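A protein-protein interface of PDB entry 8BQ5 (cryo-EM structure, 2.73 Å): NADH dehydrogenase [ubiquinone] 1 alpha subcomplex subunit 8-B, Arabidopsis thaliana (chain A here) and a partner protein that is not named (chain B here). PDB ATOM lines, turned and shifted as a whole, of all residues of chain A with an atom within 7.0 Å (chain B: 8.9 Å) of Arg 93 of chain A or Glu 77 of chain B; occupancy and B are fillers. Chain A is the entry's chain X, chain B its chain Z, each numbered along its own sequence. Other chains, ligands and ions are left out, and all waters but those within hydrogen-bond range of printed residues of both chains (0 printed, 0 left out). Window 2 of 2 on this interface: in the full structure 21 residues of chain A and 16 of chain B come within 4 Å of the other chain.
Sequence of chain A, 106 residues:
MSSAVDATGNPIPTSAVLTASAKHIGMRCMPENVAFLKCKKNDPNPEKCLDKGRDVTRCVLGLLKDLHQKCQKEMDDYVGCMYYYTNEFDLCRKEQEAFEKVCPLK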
ATOM      1  N   LYS A  23      24.243 -22.905 -18.101  1.00  0.00           N
ATOM      2  CA  LYS A  23      23.211 -21.891 -17.896  1.00  0.00           C
ATOM      3  C   LYS A  23      23.500 -21.051 -16.653  1.00  0.00           C
ATOM      4  O   LYS A  23      23.415 -19.815 -16.687  1.00  0.00           O
ATOM      5  CB  LYS A  23      21.836 -22.552 -17.808  1.00  0.00           C
ATOM      6  CG  LYS A  23      21.344 -23.129 -19.131  1.00  0.00           C
ATOM      7  CD  LYS A  23      20.013 -23.845 -18.960  1.00  0.00           C
ATOM      8  CE  LYS A  23      19.414 -24.252 -20.301  1.00  0.00           C
ATOM      9  NZ  LYS A  23      20.152 -25.376 -20.941  1.00  0.00           N
ATOM     10  N   TYR A  78      22.714 -35.178 -13.157  1.00  0.00           N
ATOM     11  CA  TYR A  78      22.697 -34.405 -14.424  1.00  0.00           C
ATOM     12  C   TYR A  78      24.051 -34.546 -15.123  1.00  0.00           C
ATOM     13  O   TYR A  78      24.067 -34.843 -16.323  1.00  0.00           O
ATOM     14  CB  TYR A  78      22.343 -32.936 -14.185  1.00  0.00           C
ATOM     15  CG  TYR A  78      21.995 -32.191 -15.449  1.00  0.00           C
ATOM     16  CD1 TYR A  78      21.417 -32.851 -16.520  1.00  0.00           C
ATOM     17  CD2 TYR A  78      22.241 -30.837 -15.579  1.00  0.00           C
ATOM     18  CE1 TYR A  78      21.100 -32.188 -17.691  1.00  0.00           C
ATOM     19  CE2 TYR A  78      21.924 -30.155 -16.742  1.00  0.00           C
ATOM     20  CZ  TYR A  78      21.356 -30.835 -17.805  1.00  0.00           C
ATOM     21  OH  TYR A  78      21.029 -30.181 -18.955  1.00  0.00           O
ATOM     22  N   CYS A  81      24.405 -37.992 -16.626  1.00  0.00           N
ATOM     23  CA  CYS A  81      23.579 -38.220 -17.842  1.00  0.00           C
ATOM     24  C   CYS A  81      24.161 -37.401 -19.000  1.00  0.00           C
ATOM     25  O   CYS A  81      24.223 -37.937 -20.123  1.00  0.00           O
ATOM     26  CB  CYS A  81      22.118 -37.866 -17.593  1.00  0.00           C
ATOM     27  SG  CYS A  81      20.980 -38.637 -18.771  1.00  0.00           S
ATOM     28  N   GLU A  88      24.377 -33.949 -24.755  1.00  0.00           N
ATOM     29  CA  GLU A  88      23.147 -33.693 -25.564  1.00  0.00           C
ATOM     30  C   GLU A  88      22.005 -33.308 -24.622  1.00  0.00           C
ATOM     31  O   GLU A  88      21.520 -34.192 -23.897  1.00  0.00           O
ATOM     32  CB  GLU A  88      22.790 -34.887 -26.454  1.00  0.00           C
ATOM     33  CG  GLU A  88      21.984 -34.490 -27.677  1.00  0.00           C
ATOM     34  CD  GLU A  88      22.680 -33.511 -28.610  1.00  0.00           C
ATOM     35  OE1 GLU A  88      23.630 -33.926 -29.292  1.00  0.00           O
ATOM     36  OE2 GLU A  88      22.273 -32.332 -28.649  1.00  0.00           O
ATOM     37  N   PHE A  89      21.580 -32.041 -24.646  1.00  0.00           N
ATOM     38  CA  PHE A  89      20.578 -31.578 -23.689  1.00  0.00           C
ATOM     39  C   PHE A  89      19.265 -32.344 -23.821  1.00  0.00           C
ATOM     40  O   PHE A  89      18.566 -32.562 -22.826  1.00  0.00           O
ATOM     41  CB  PHE A  89      20.330 -30.077 -23.855  1.00  0.00           C
ATOM     42  CG  PHE A  89      21.507 -29.219 -23.492  1.00  0.00           C
ATOM     43  CD1 PHE A  89      21.697 -28.803 -22.185  1.00  0.00           C
ATOM     44  CD2 PHE A  89      22.409 -28.809 -24.457  1.00  0.00           C
ATOM     45  CE1 PHE A  89      22.770 -28.009 -21.847  1.00  0.00           C
ATOM     46  CE2 PHE A  89      23.485 -28.016 -24.123  1.00  0.00           C
ATOM     47  CZ  PHE A  89      23.665 -27.622 -22.813  1.00  0.00           C
ATOM     48  N   ASP A  90      18.911 -32.757 -25.040  1.00  0.00           N
ATOM     49  CA  ASP A  90      17.586 -33.332 -25.265  1.00  0.00           C
ATOM     50  C   ASP A  90      17.437 -34.693 -24.597  1.00  0.00           C
ATOM     51  O   ASP A  90      16.325 -35.092 -24.230  1.00  0.00           O
ATOM     52  CB  ASP A  90      17.304 -33.441 -26.762  1.00  0.00           C
ATOM     53  CG  ASP A  90      17.079 -32.088 -27.407  1.00  0.00           C
ATOM     54  OD1 ASP A  90      16.858 -31.106 -26.670  1.00  0.00           O
ATOM     55  OD2 ASP A  90      17.111 -32.011 -28.653  1.00  0.00           O
ATOM     56  N   LEU A  91      18.533 -35.426 -24.435  1.00  0.00           N
ATOM     57  CA  LEU A  91      18.479 -36.741 -23.810  1.00  0.00           C
ATOM     58  C   LEU A  91      18.629 -36.685 -22.295  1.00  0.00           C
ATOM     59  O   LEU A  91      18.787 -37.735 -21.664  1.00  0.00           O
ATOM     60  CB  LEU A  91      19.555 -37.650 -24.411  1.00  0.00           C
ATOM     61  CG  LEU A  91      19.438 -37.872 -25.920  1.00  0.00           C
ATOM     62  CD1 LEU A  91      20.776 -38.235 -26.535  1.00  0.00           C
ATOM     63  CD2 LEU A  91      18.410 -38.950 -26.206  1.00  0.00           C
ATOM     64  N   CYS A  92      18.569 -35.488 -21.699  1.00  0.00           N
ATOM     65  CA  CYS A  92      18.823 -35.335 -20.271  1.00  0.00           C
ATOM     66  C   CYS A  92      17.831 -34.392 -19.598  1.00  0.00           C
ATOM     67  O   CYS A  92      18.183 -33.750 -18.601  1.00  0.00           O
ATOM     68  CB  CYS A  92      20.242 -34.805 -20.030  1.00  0.00           C
ATOM     69  SG  CYS A  92      21.574 -35.785 -20.751  1.00  0.00           S
ATOM     70  N   ARG A  93      16.605 -34.287 -20.114  1.00  0.00           N
ATOM     71  CA  ARG A  93      15.692 -33.240 -19.659  1.00  0.00           C
ATOM     72  C   ARG A  93      15.246 -33.455 -18.217  1.00  0.00           C
ATOM     73  O   ARG A  93      15.194 -32.500 -17.433  1.00  0.00           O
ATOM     74  CB  ARG A  93      14.482 -33.166 -20.587  1.00  0.00           C
ATOM     75  CG  ARG A  93      14.818 -32.715 -21.995  1.00  0.00           C
ATOM     76  CD  ARG A  93      15.241 -31.257 -22.019  1.00  0.00           C
ATOM     77  NE  ARG A  93      15.507 -30.792 -23.375  1.00  0.00           N
ATOM     78  CZ  ARG A  93      16.337 -29.804 -23.679  1.00  0.00           C
ATOM     79  NH1 ARG A  93      16.999 -29.145 -22.743  1.00  0.00           N
ATOM     80  NH2 ARG A  93      16.508 -29.470 -24.954  1.00  0.00           N
ATOM     81  N   LYS A  94      14.908 -34.694 -17.849  1.00  0.00           N
ATOM     82  CA  LYS A  94      14.371 -34.945 -16.514  1.00  0.00           C
ATOM     83  C   LYS A  94      15.393 -34.598 -15.439  1.00  0.00           C
ATOM     84  O   LYS A  94      15.065 -33.963 -14.428  1.00  0.00           O
ATOM     85  CB  LYS A  94      13.907 -36.402 -16.397  1.00  0.00           C
ATOM     86  CG  LYS A  94      15.025 -37.437 -16.320  1.00  0.00           C
ATOM     87  CD  LYS A  94      14.509 -38.834 -16.019  1.00  0.00           C
ATOM     88  CE  LYS A  94      13.363 -38.818 -15.026  1.00  0.00           C
ATOM     89  NZ  LYS A  94      13.397 -40.020 -14.150  1.00  0.00           N
ATOM     90  N   GLU A  95      16.653 -34.977 -15.657  1.00  0.00           N
ATOM     91  CA  GLU A  95      17.697 -34.608 -14.715  1.00  0.00           C
ATOM     92  C   GLU A  95      17.986 -33.115 -14.774  1.00  0.00           C
ATOM     93  O   GLU A  95      18.315 -32.515 -13.749  1.00  0.00           O
ATOM     94  CB  GLU A  95      18.949 -35.441 -14.979  1.00  0.00           C
ATOM     95  CG  GLU A  95      18.760 -36.902 -14.596  1.00  0.00           C
ATOM     96  CD  GLU A  95      18.549 -37.811 -15.792  1.00  0.00           C
ATOM     97  OE1 GLU A  95      18.193 -37.305 -16.876  1.00  0.00           O
ATOM     98  OE2 GLU A  95      18.719 -39.039 -15.640  1.00  0.00           O
ATOM     99  N   GLN A  96      17.816 -32.492 -15.944  1.00  0.00           N
ATOM    100  CA  GLN A  96      17.928 -31.037 -16.022  1.00  0.00           C
ATOM    101  C   GLN A  96      16.871 -30.352 -15.167  1.00  0.00           C
ATOM    102  O   GLN A  96      17.176 -29.409 -14.429  1.00  0.00           O
ATOM    103  CB  GLN A  96      17.812 -30.569 -17.472  1.00  0.00           C
ATOM    104  CG  GLN A  96      17.676 -29.056 -17.611  1.00  0.00           C
ATOM    105  CD  GLN A  96      17.783 -28.581 -19.045  1.00  0.00           C
ATOM    106  OE1 GLN A  96      18.179 -29.335 -19.933  1.00  0.00           O
ATOM    107  NE2 GLN A  96      17.429 -27.323 -19.280  1.00  0.00           N
ATOM    108  N   GLU A  97      15.616 -30.799 -15.266  1.00  0.00           N
ATOM    109  CA  GLU A  97      14.555 -30.183 -14.475  1.00  0.00           C
ATOM    110  C   GLU A  97      14.774 -30.420 -12.988  1.00  0.00           C
ATOM    111  O   GLU A  97      14.607 -29.502 -12.176  1.00  0.00           O
ATOM    112  CB  GLU A  97      13.190 -30.717 -14.911  1.00  0.00           C
ATOM    113  CG  GLU A  97      12.023 -29.867 -14.434  1.00  0.00           C
ATOM    114  CD  GLU A  97      11.382 -30.407 -13.169  1.00  0.00           C
ATOM    115  OE1 GLU A  97      10.924 -29.595 -12.339  1.00  0.00           O
ATOM    116  OE2 GLU A  97      11.332 -31.645 -13.009  1.00  0.00           O
ATOM    117  N   ALA A  98      15.161 -31.642 -12.613  1.00  0.00           N
ATOM    118  CA  ALA A  98      15.443 -31.927 -11.209  1.00  0.00           C
ATOM    119  C   ALA A  98      16.611 -31.090 -10.698  1.00  0.00           C
ATOM    120  O   ALA A  98      16.643 -30.706  -9.524  1.00  0.00           O
ATOM    121  CB  ALA A  98      15.725 -33.417 -11.023  1.00  0.00           C
ATOM    122  N   PHE A  99      17.580 -30.801 -11.568  1.00  0.00           N
ATOM    123  CA  PHE A  99      18.730 -29.993 -11.186  1.00  0.00           C
ATOM    124  C   PHE A  99      18.350 -28.528 -11.002  1.00  0.00           C
ATOM    125  O   PHE A  99      18.741 -27.900 -10.011  1.00  0.00           O
ATOM    126  CB  PHE A  99      19.821 -30.159 -12.245  1.00  0.00           C
ATOM    127  CG  PHE A  99      20.969 -29.206 -12.111  1.00  0.00           C
ATOM    128  CD1 PHE A  99      21.800 -29.242 -11.007  1.00  0.00           C
ATOM    129  CD2 PHE A  99      21.243 -28.302 -13.121  1.00  0.00           C
ATOM    130  CE1 PHE A  99      22.862 -28.373 -10.903  1.00  0.00           C
ATOM    131  CE2 PHE A  99      22.304 -27.434 -13.022  1.00  0.00           C
ATOM    132  CZ  PHE A  99      23.112 -27.473 -11.915  1.00  0.00           C
ATOM    133  N   ILE B  70      11.471 -25.653 -34.064  1.00  0.00           N
ATOM    134  CA  ILE B  70      11.862 -26.384 -32.824  1.00  0.00           C
ATOM    135  C   ILE B  70      13.297 -26.917 -32.952  1.00  0.00           C
ATOM    136  O   ILE B  70      14.063 -26.744 -31.999  1.00  0.00           O
ATOM    137  CB  ILE B  70      10.838 -27.502 -32.537  1.00  0.00           C
ATOM    138  CG1 ILE B  70       9.449 -26.932 -32.238  1.00  0.00           C
ATOM    139  CG2 ILE B  70      11.311 -28.429 -31.428  1.00  0.00           C
ATOM    140  CD1 ILE B  70       8.328 -27.927 -32.417  1.00  0.00           C
ATOM    141  N   ARG B  71      13.653 -27.526 -34.089  1.00  0.00           N
ATOM    142  CA  ARG B  71      15.035 -28.030 -34.308  1.00  0.00           C
ATOM    143  C   ARG B  71      16.035 -26.878 -34.142  1.00  0.00           C
ATOM    144  O   ARG B  71      17.044 -27.090 -33.462  1.00  0.00           O
ATOM    145  CB  ARG B  71      15.156 -28.694 -35.679  1.00  0.00           C
ATOM    146  CG  ARG B  71      14.993 -30.203 -35.672  1.00  0.00           C
ATOM    147  CD  ARG B  71      15.725 -30.785 -36.860  1.00  0.00           C
ATOM    148  NE  ARG B  71      15.289 -30.258 -38.146  1.00  0.00           N
ATOM    149  CZ  ARG B  71      16.092 -30.019 -39.177  1.00  0.00           C
ATOM    150  NH1 ARG B  71      17.390 -30.248 -39.081  1.00  0.00           N
ATOM    151  NH2 ARG B  71      15.594 -29.551 -40.305  1.00  0.00           N
ATOM    152  N   ARG B  72      15.744 -25.706 -34.709  1.00  0.00           N
ATOM    153  CA  ARG B  72      16.625 -24.511 -34.581  1.00  0.00           C
ATOM    154  C   ARG B  72      16.772 -24.102 -33.111  1.00  0.00           C
ATOM    155  O   ARG B  72      17.886 -23.743 -32.732  1.00  0.00           O
ATOM    156  CB  ARG B  72      16.044 -23.341 -35.374  1.00  0.00           C
ATOM    157  CG  ARG B  72      17.047 -22.598 -36.242  1.00  0.00           C
ATOM    158  CD  ARG B  72      16.446 -22.176 -37.570  1.00  0.00           C
ATOM    159  NE  ARG B  72      15.320 -21.263 -37.434  1.00  0.00           N
ATOM    160  CZ  ARG B  72      14.090 -21.491 -37.890  1.00  0.00           C
ATOM    161  NH1 ARG B  72      13.808 -22.620 -38.516  1.00  0.00           N
ATOM    162  NH2 ARG B  72      13.146 -20.586 -37.711  1.00  0.00           N
ATOM    163  N   ALA B  73      15.687 -24.138 -32.333  1.00  0.00           N
ATOM    164  CA  ALA B  73      15.744 -23.795 -30.893  1.00  0.00           C
ATOM    165  C   ALA B  73      16.689 -24.744 -30.145  1.00  0.00           C
ATOM    166  O   ALA B  73      17.483 -24.246 -29.344  1.00  0.00           O
ATOM    167  CB  ALA B  73      14.366 -23.811 -30.289  1.00  0.00           C
ATOM    168  N   LEU B  74      16.572 -26.056 -30.371  1.00  0.00           N
ATOM    169  CA  LEU B  74      17.425 -27.037 -29.648  1.00  0.00           C
ATOM    170  C   LEU B  74      18.886 -26.768 -30.005  1.00  0.00           C
ATOM    171  O   LEU B  74      19.733 -26.867 -29.107  1.00  0.00           O
ATOM    172  CB  LEU B  74      17.044 -28.462 -30.044  1.00  0.00           C
ATOM    173  CG  LEU B  74      15.578 -28.843 -29.876  1.00  0.00           C
ATOM    174  CD1 LEU B  74      15.314 -30.197 -30.513  1.00  0.00           C
ATOM    175  CD2 LEU B  74      15.185 -28.854 -28.408  1.00  0.00           C
ATOM    176  N   LYS B  75      19.160 -26.448 -31.269  1.00  0.00           N
ATOM    177  CA  LYS B  75      20.543 -26.141 -31.705  1.00  0.00           C
ATOM    178  C   LYS B  75      20.996 -24.821 -31.080  1.00  0.00           C
ATOM    179  O   LYS B  75      22.145 -24.765 -30.644  1.00  0.00           O
ATOM    180  CB  LYS B  75      20.622 -26.073 -33.232  1.00  0.00           C
ATOM    181  CG  LYS B  75      20.251 -27.361 -33.947  1.00  0.00           C
ATOM    182  CD  LYS B  75      21.194 -28.501 -33.646  1.00  0.00           C
ATOM    183  CE  LYS B  75      20.858 -29.759 -34.419  1.00  0.00           C
ATOM    184  NZ  LYS B  75      21.781 -30.873 -34.094  1.00  0.00           N
ATOM    185  N   GLU B  76      20.131 -23.811 -31.063  1.00  0.00           N
ATOM    186  CA  GLU B  76      20.468 -22.506 -30.438  1.00  0.00           C
ATOM    187  C   GLU B  76      20.801 -22.746 -28.971  1.00  0.00           C
ATOM    188  O   GLU B  76      21.770 -22.135 -28.499  1.00  0.00           O
ATOM    189  CB  GLU B  76      19.312 -21.518 -30.580  1.00  0.00           C
ATOM    190  CG  GLU B  76      19.772 -20.104 -30.875  1.00  0.00           C
ATOM    191  CD  GLU B  76      20.910 -19.994 -31.876  1.00  0.00           C
ATOM    192  OE1 GLU B  76      22.033 -19.635 -31.457  1.00  0.00           O
ATOM    193  OE2 GLU B  76      20.671 -20.253 -33.075  1.00  0.00           O
ATOM    194  N   GLU B  77      19.999 -23.554 -28.280  1.00  0.00           N
ATOM    195  CA  GLU B  77      20.328 -23.926 -26.909  1.00  0.00           C
ATOM    196  C   GLU B  77      21.752 -24.458 -26.814  1.00  0.00           C
ATOM    197  O   GLU B  77      22.533 -24.038 -25.948  1.00  0.00           O
ATOM    198  CB  GLU B  77      19.338 -24.972 -26.399  1.00  0.00           C
ATOM    199  CG  GLU B  77      19.933 -25.927 -25.375  1.00  0.00           C
ATOM    200  CD  GLU B  77      18.907 -26.459 -24.400  1.00  0.00           C
ATOM    201  OE1 GLU B  77      19.190 -26.459 -23.185  1.00  0.00           O
ATOM    202  OE2 GLU B  77      17.825 -26.890 -24.851  1.00  0.00           O
ATOM    203  N   LYS B  78      22.106 -25.395 -27.700  1.00  0.00           N
ATOM    204  CA  LYS B  78      23.444 -25.978 -27.632  1.00  0.00           C
ATOM    205  C   LYS B  78      24.521 -24.918 -27.851  1.00  0.00           C
ATOM    206  O   LYS B  78      25.512 -24.853 -27.106  1.00  0.00           O
ATOM    207  CB  LYS B  78      23.587 -27.103 -28.657  1.00  0.00           C
ATOM    208  CG  LYS B  78      24.932 -27.808 -28.597  1.00  0.00           C
ATOM    209  CD  LYS B  78      25.034 -28.913 -29.626  1.00  0.00           C
ATOM    210  CE  LYS B  78      25.068 -28.359 -31.036  1.00  0.00           C
ATOM    211  NZ  LYS B  78      26.296 -27.552 -31.268  1.00  0.00           N
ATOM    212  N   TYR B  79      24.326 -24.060 -28.851  1.00  0.00           N
ATOM    213  CA  TYR B  79      25.299 -23.017 -29.157  1.00  0.00           C
ATOM    214  C   TYR B  79      25.418 -22.011 -28.017  1.00  0.00           C
ATOM    215  O   TYR B  79      26.517 -21.526 -27.728  1.00  0.00           O
ATOM    216  CB  TYR B  79      24.912 -22.313 -30.456  1.00  0.00           C
ATOM    217  CG  TYR B  79      25.010 -23.205 -31.673  1.00  0.00           C
ATOM    218  CD1 TYR B  79      25.985 -24.189 -31.760  1.00  0.00           C
ATOM    219  CD2 TYR B  79      24.118 -23.071 -32.729  1.00  0.00           C
ATOM    220  CE1 TYR B  79      26.073 -25.008 -32.865  1.00  0.00           C
ATOM    221  CE2 TYR B  79      24.198 -23.887 -33.838  1.00  0.00           C
ATOM    222  CZ  TYR B  79      25.178 -24.853 -33.902  1.00  0.00           C
ATOM    223  OH  TYR B  79      25.268 -25.668 -35.005  1.00  0.00           O
ATOM    224  N   ALA B  80      24.298 -21.682 -27.368  1.00  0.00           N
ATOM    225  CA  ALA B  80      24.340 -20.785 -26.219  1.00  0.00           C
ATOM    226  C   ALA B  80      25.118 -21.406 -25.069  1.00  0.00           C
ATOM    227  O   ALA B  80      25.884 -20.718 -24.387  1.00  0.00           O
ATOM    228  CB  ALA B  80      22.921 -20.432 -25.776  1.00  0.00           C
ATOM    229  N   ALA B  81      24.930 -22.705 -24.834  1.00  0.00           N
ATOM    230  CA  ALA B  81      25.706 -23.376 -23.796  1.00  0.00           C
ATOM    231  C   ALA B  81      27.191 -23.369 -24.130  1.00  0.00           C
ATOM    232  O   ALA B  81      28.038 -23.305 -23.232  1.00  0.00           O
ATOM    233  CB  ALA B  81      25.212 -24.805 -23.606  1.00  0.00           C
ATOM    234  N   ARG B  82      27.528 -23.447 -25.418  1.00  0.00           N
ATOM    235  CA  ARG B  82      28.933 -23.368 -25.803  1.00  0.00           C
ATOM    236  C   ARG B  82      29.503 -21.972 -25.582  1.00  0.00           C
ATOM    237  O   ARG B  82      30.693 -21.829 -25.285  1.00  0.00           O
ATOM    238  CB  ARG B  82      29.101 -23.784 -27.260  1.00  0.00           C
ATOM    239  CG  ARG B  82      29.178 -25.280 -27.436  1.00  0.00           C
ATOM    240  CD  ARG B  82      29.080 -25.676 -28.884  1.00  0.00           C
ATOM    241  NE  ARG B  82      29.096 -27.126 -29.027  1.00  0.00           N
ATOM    242  CZ  ARG B  82      29.115 -27.762 -30.189  1.00  0.00           C
ATOM    243  NH1 ARG B  82      29.117 -27.106 -31.336  1.00  0.00           N
ATOM    244  NH2 ARG B  82      29.135 -29.091 -30.199  1.00  0.00           N
ATOM    245  N   ARG B  83      28.674 -20.937 -25.722  1.00  0.00           N
ATOM    246  CA  ARG B  83      29.180 -19.572 -25.634  1.00  0.00           C
ATOM    247  C   ARG B  83      29.433 -19.137 -24.195  1.00  0.00           C
ATOM    248  O   ARG B  83      30.301 -18.292 -23.954  1.00  0.00           O
ATOM    249  CB  ARG B  83      28.207 -18.618 -26.326  1.00  0.00           C
ATOM    250  CG  ARG B  83      28.489 -18.455 -27.810  1.00  0.00           C
ATOM    251  CD  ARG B  83      27.690 -17.319 -28.411  1.00  0.00           C
ATOM    252  NE  ARG B  83      26.261 -17.599 -28.364  1.00  0.00           N
ATOM    253  CZ  ARG B  83      25.573 -18.139 -29.361  1.00  0.00           C
ATOM    254  NH1 ARG B  83      26.149 -18.447 -30.512  1.00  0.00           N
ATOM    255  NH2 ARG B  83      24.275 -18.374 -29.199  1.00  0.00           N
ATOM    256  N   THR B  84      28.691 -19.685 -23.231  1.00  0.00           N
ATOM    257  CA  THR B  84      28.866 -19.265 -21.844  1.00  0.00           C
ATOM    258  C   THR B  84      30.102 -19.877 -21.199  1.00  0.00           C
ATOM    259  O   THR B  84      30.662 -19.288 -20.268  1.00  0.00           O
ATOM    260  CB  THR B  84      27.628 -19.611 -21.017  1.00  0.00           C
ATOM    261  OG1 THR B  84      27.543 -21.030 -20.844  1.00  0.00           O
ATOM    262  CG2 THR B  84      26.375 -19.110 -21.705  1.00  0.00           C
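Phe 89 of chain A touches Glu 77 of chain B (CD1 to OE1, 3.6 Å).
Ala 81 of chain B touches Phe 89 of chain A (CB to CZ, 3.3 Å).
OD2 of Asp 90 of chain A touches CD1 of Leu 74 of chain B, 3.2 Å away.
Arg 93 of chain A touches Leu 74 of chain B.
Printed residues of chain B within 4 Å of Lys 23 of chain A: Glu 77.
Of the printed residues of chain B, Phe 89 of chain A touches Glu 77 and Ala 81.
Asp 90 of chain A touches just one residue of chain B: Leu 74 (3.2 Å).
Arg 93 of chain A touches two residues of chain B.
Of the printed residues of chain A, Leu 74 of chain B touches Asp 90 (3.2 Å) and Arg 93 (3.7 Å).
Of chain A, only Lys 23 (2.7 Å), Phe 89 (3.6 Å) and Arg 93 (2.9 Å) come within 4 Å of Glu 77 of chain B.
The nearest residue of chain B that does not touch Arg 93 of chain A is Ala 73 of chain B (6.9 Å).
The nearest residue of chain A that does not touch Glu 77 of chain B is Gln 96 of chain A (4.4 Å).
The nearest printed residue of chain B that does not touch Lys 23 of chain A is Thr 84 of chain B (4.7 Å).
The guanidinium group of Arg 93 of chain A lies within salt-bridge range of the side-chain carboxylate of Glu 77 of chain B (2.9 Å).
The side-chain carboxylate (OE1) of Glu 77 of chain B is in salt-bridge range of the side-chain amino group (NZ) of Lys 23 of chain A, 2.7 Å away.
Hydrophobic or aromatic side chains of chain B within 4 Å of the printed part of chain A: Leu 74 and Ala 81.
Hydrophobic or aromatic side chains of chain A within 4 Å of the printed part of chain B: Phe 89.
Among the printed residues, 6 pairs touch across the chains.
The side-chain hydroxyl (OG1) of Thr 84 of chain B sits at hydrogen-bond distance from the backbone carbonyl oxygen (O) of Ala 81 of chain B, at 3.3 Å.
The side-chain carboxylate (OD1) of Asp 90 of chain A is in salt-bridge range of the guanidinium group (NE) of Arg 93 of chain A, 3.6 Å away.
The side-chain amide oxygen of Gln 96 of chain A lies within hydrogen-bond range of the guanidinium group of Arg 93 of chain A, 3.1 Å away.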
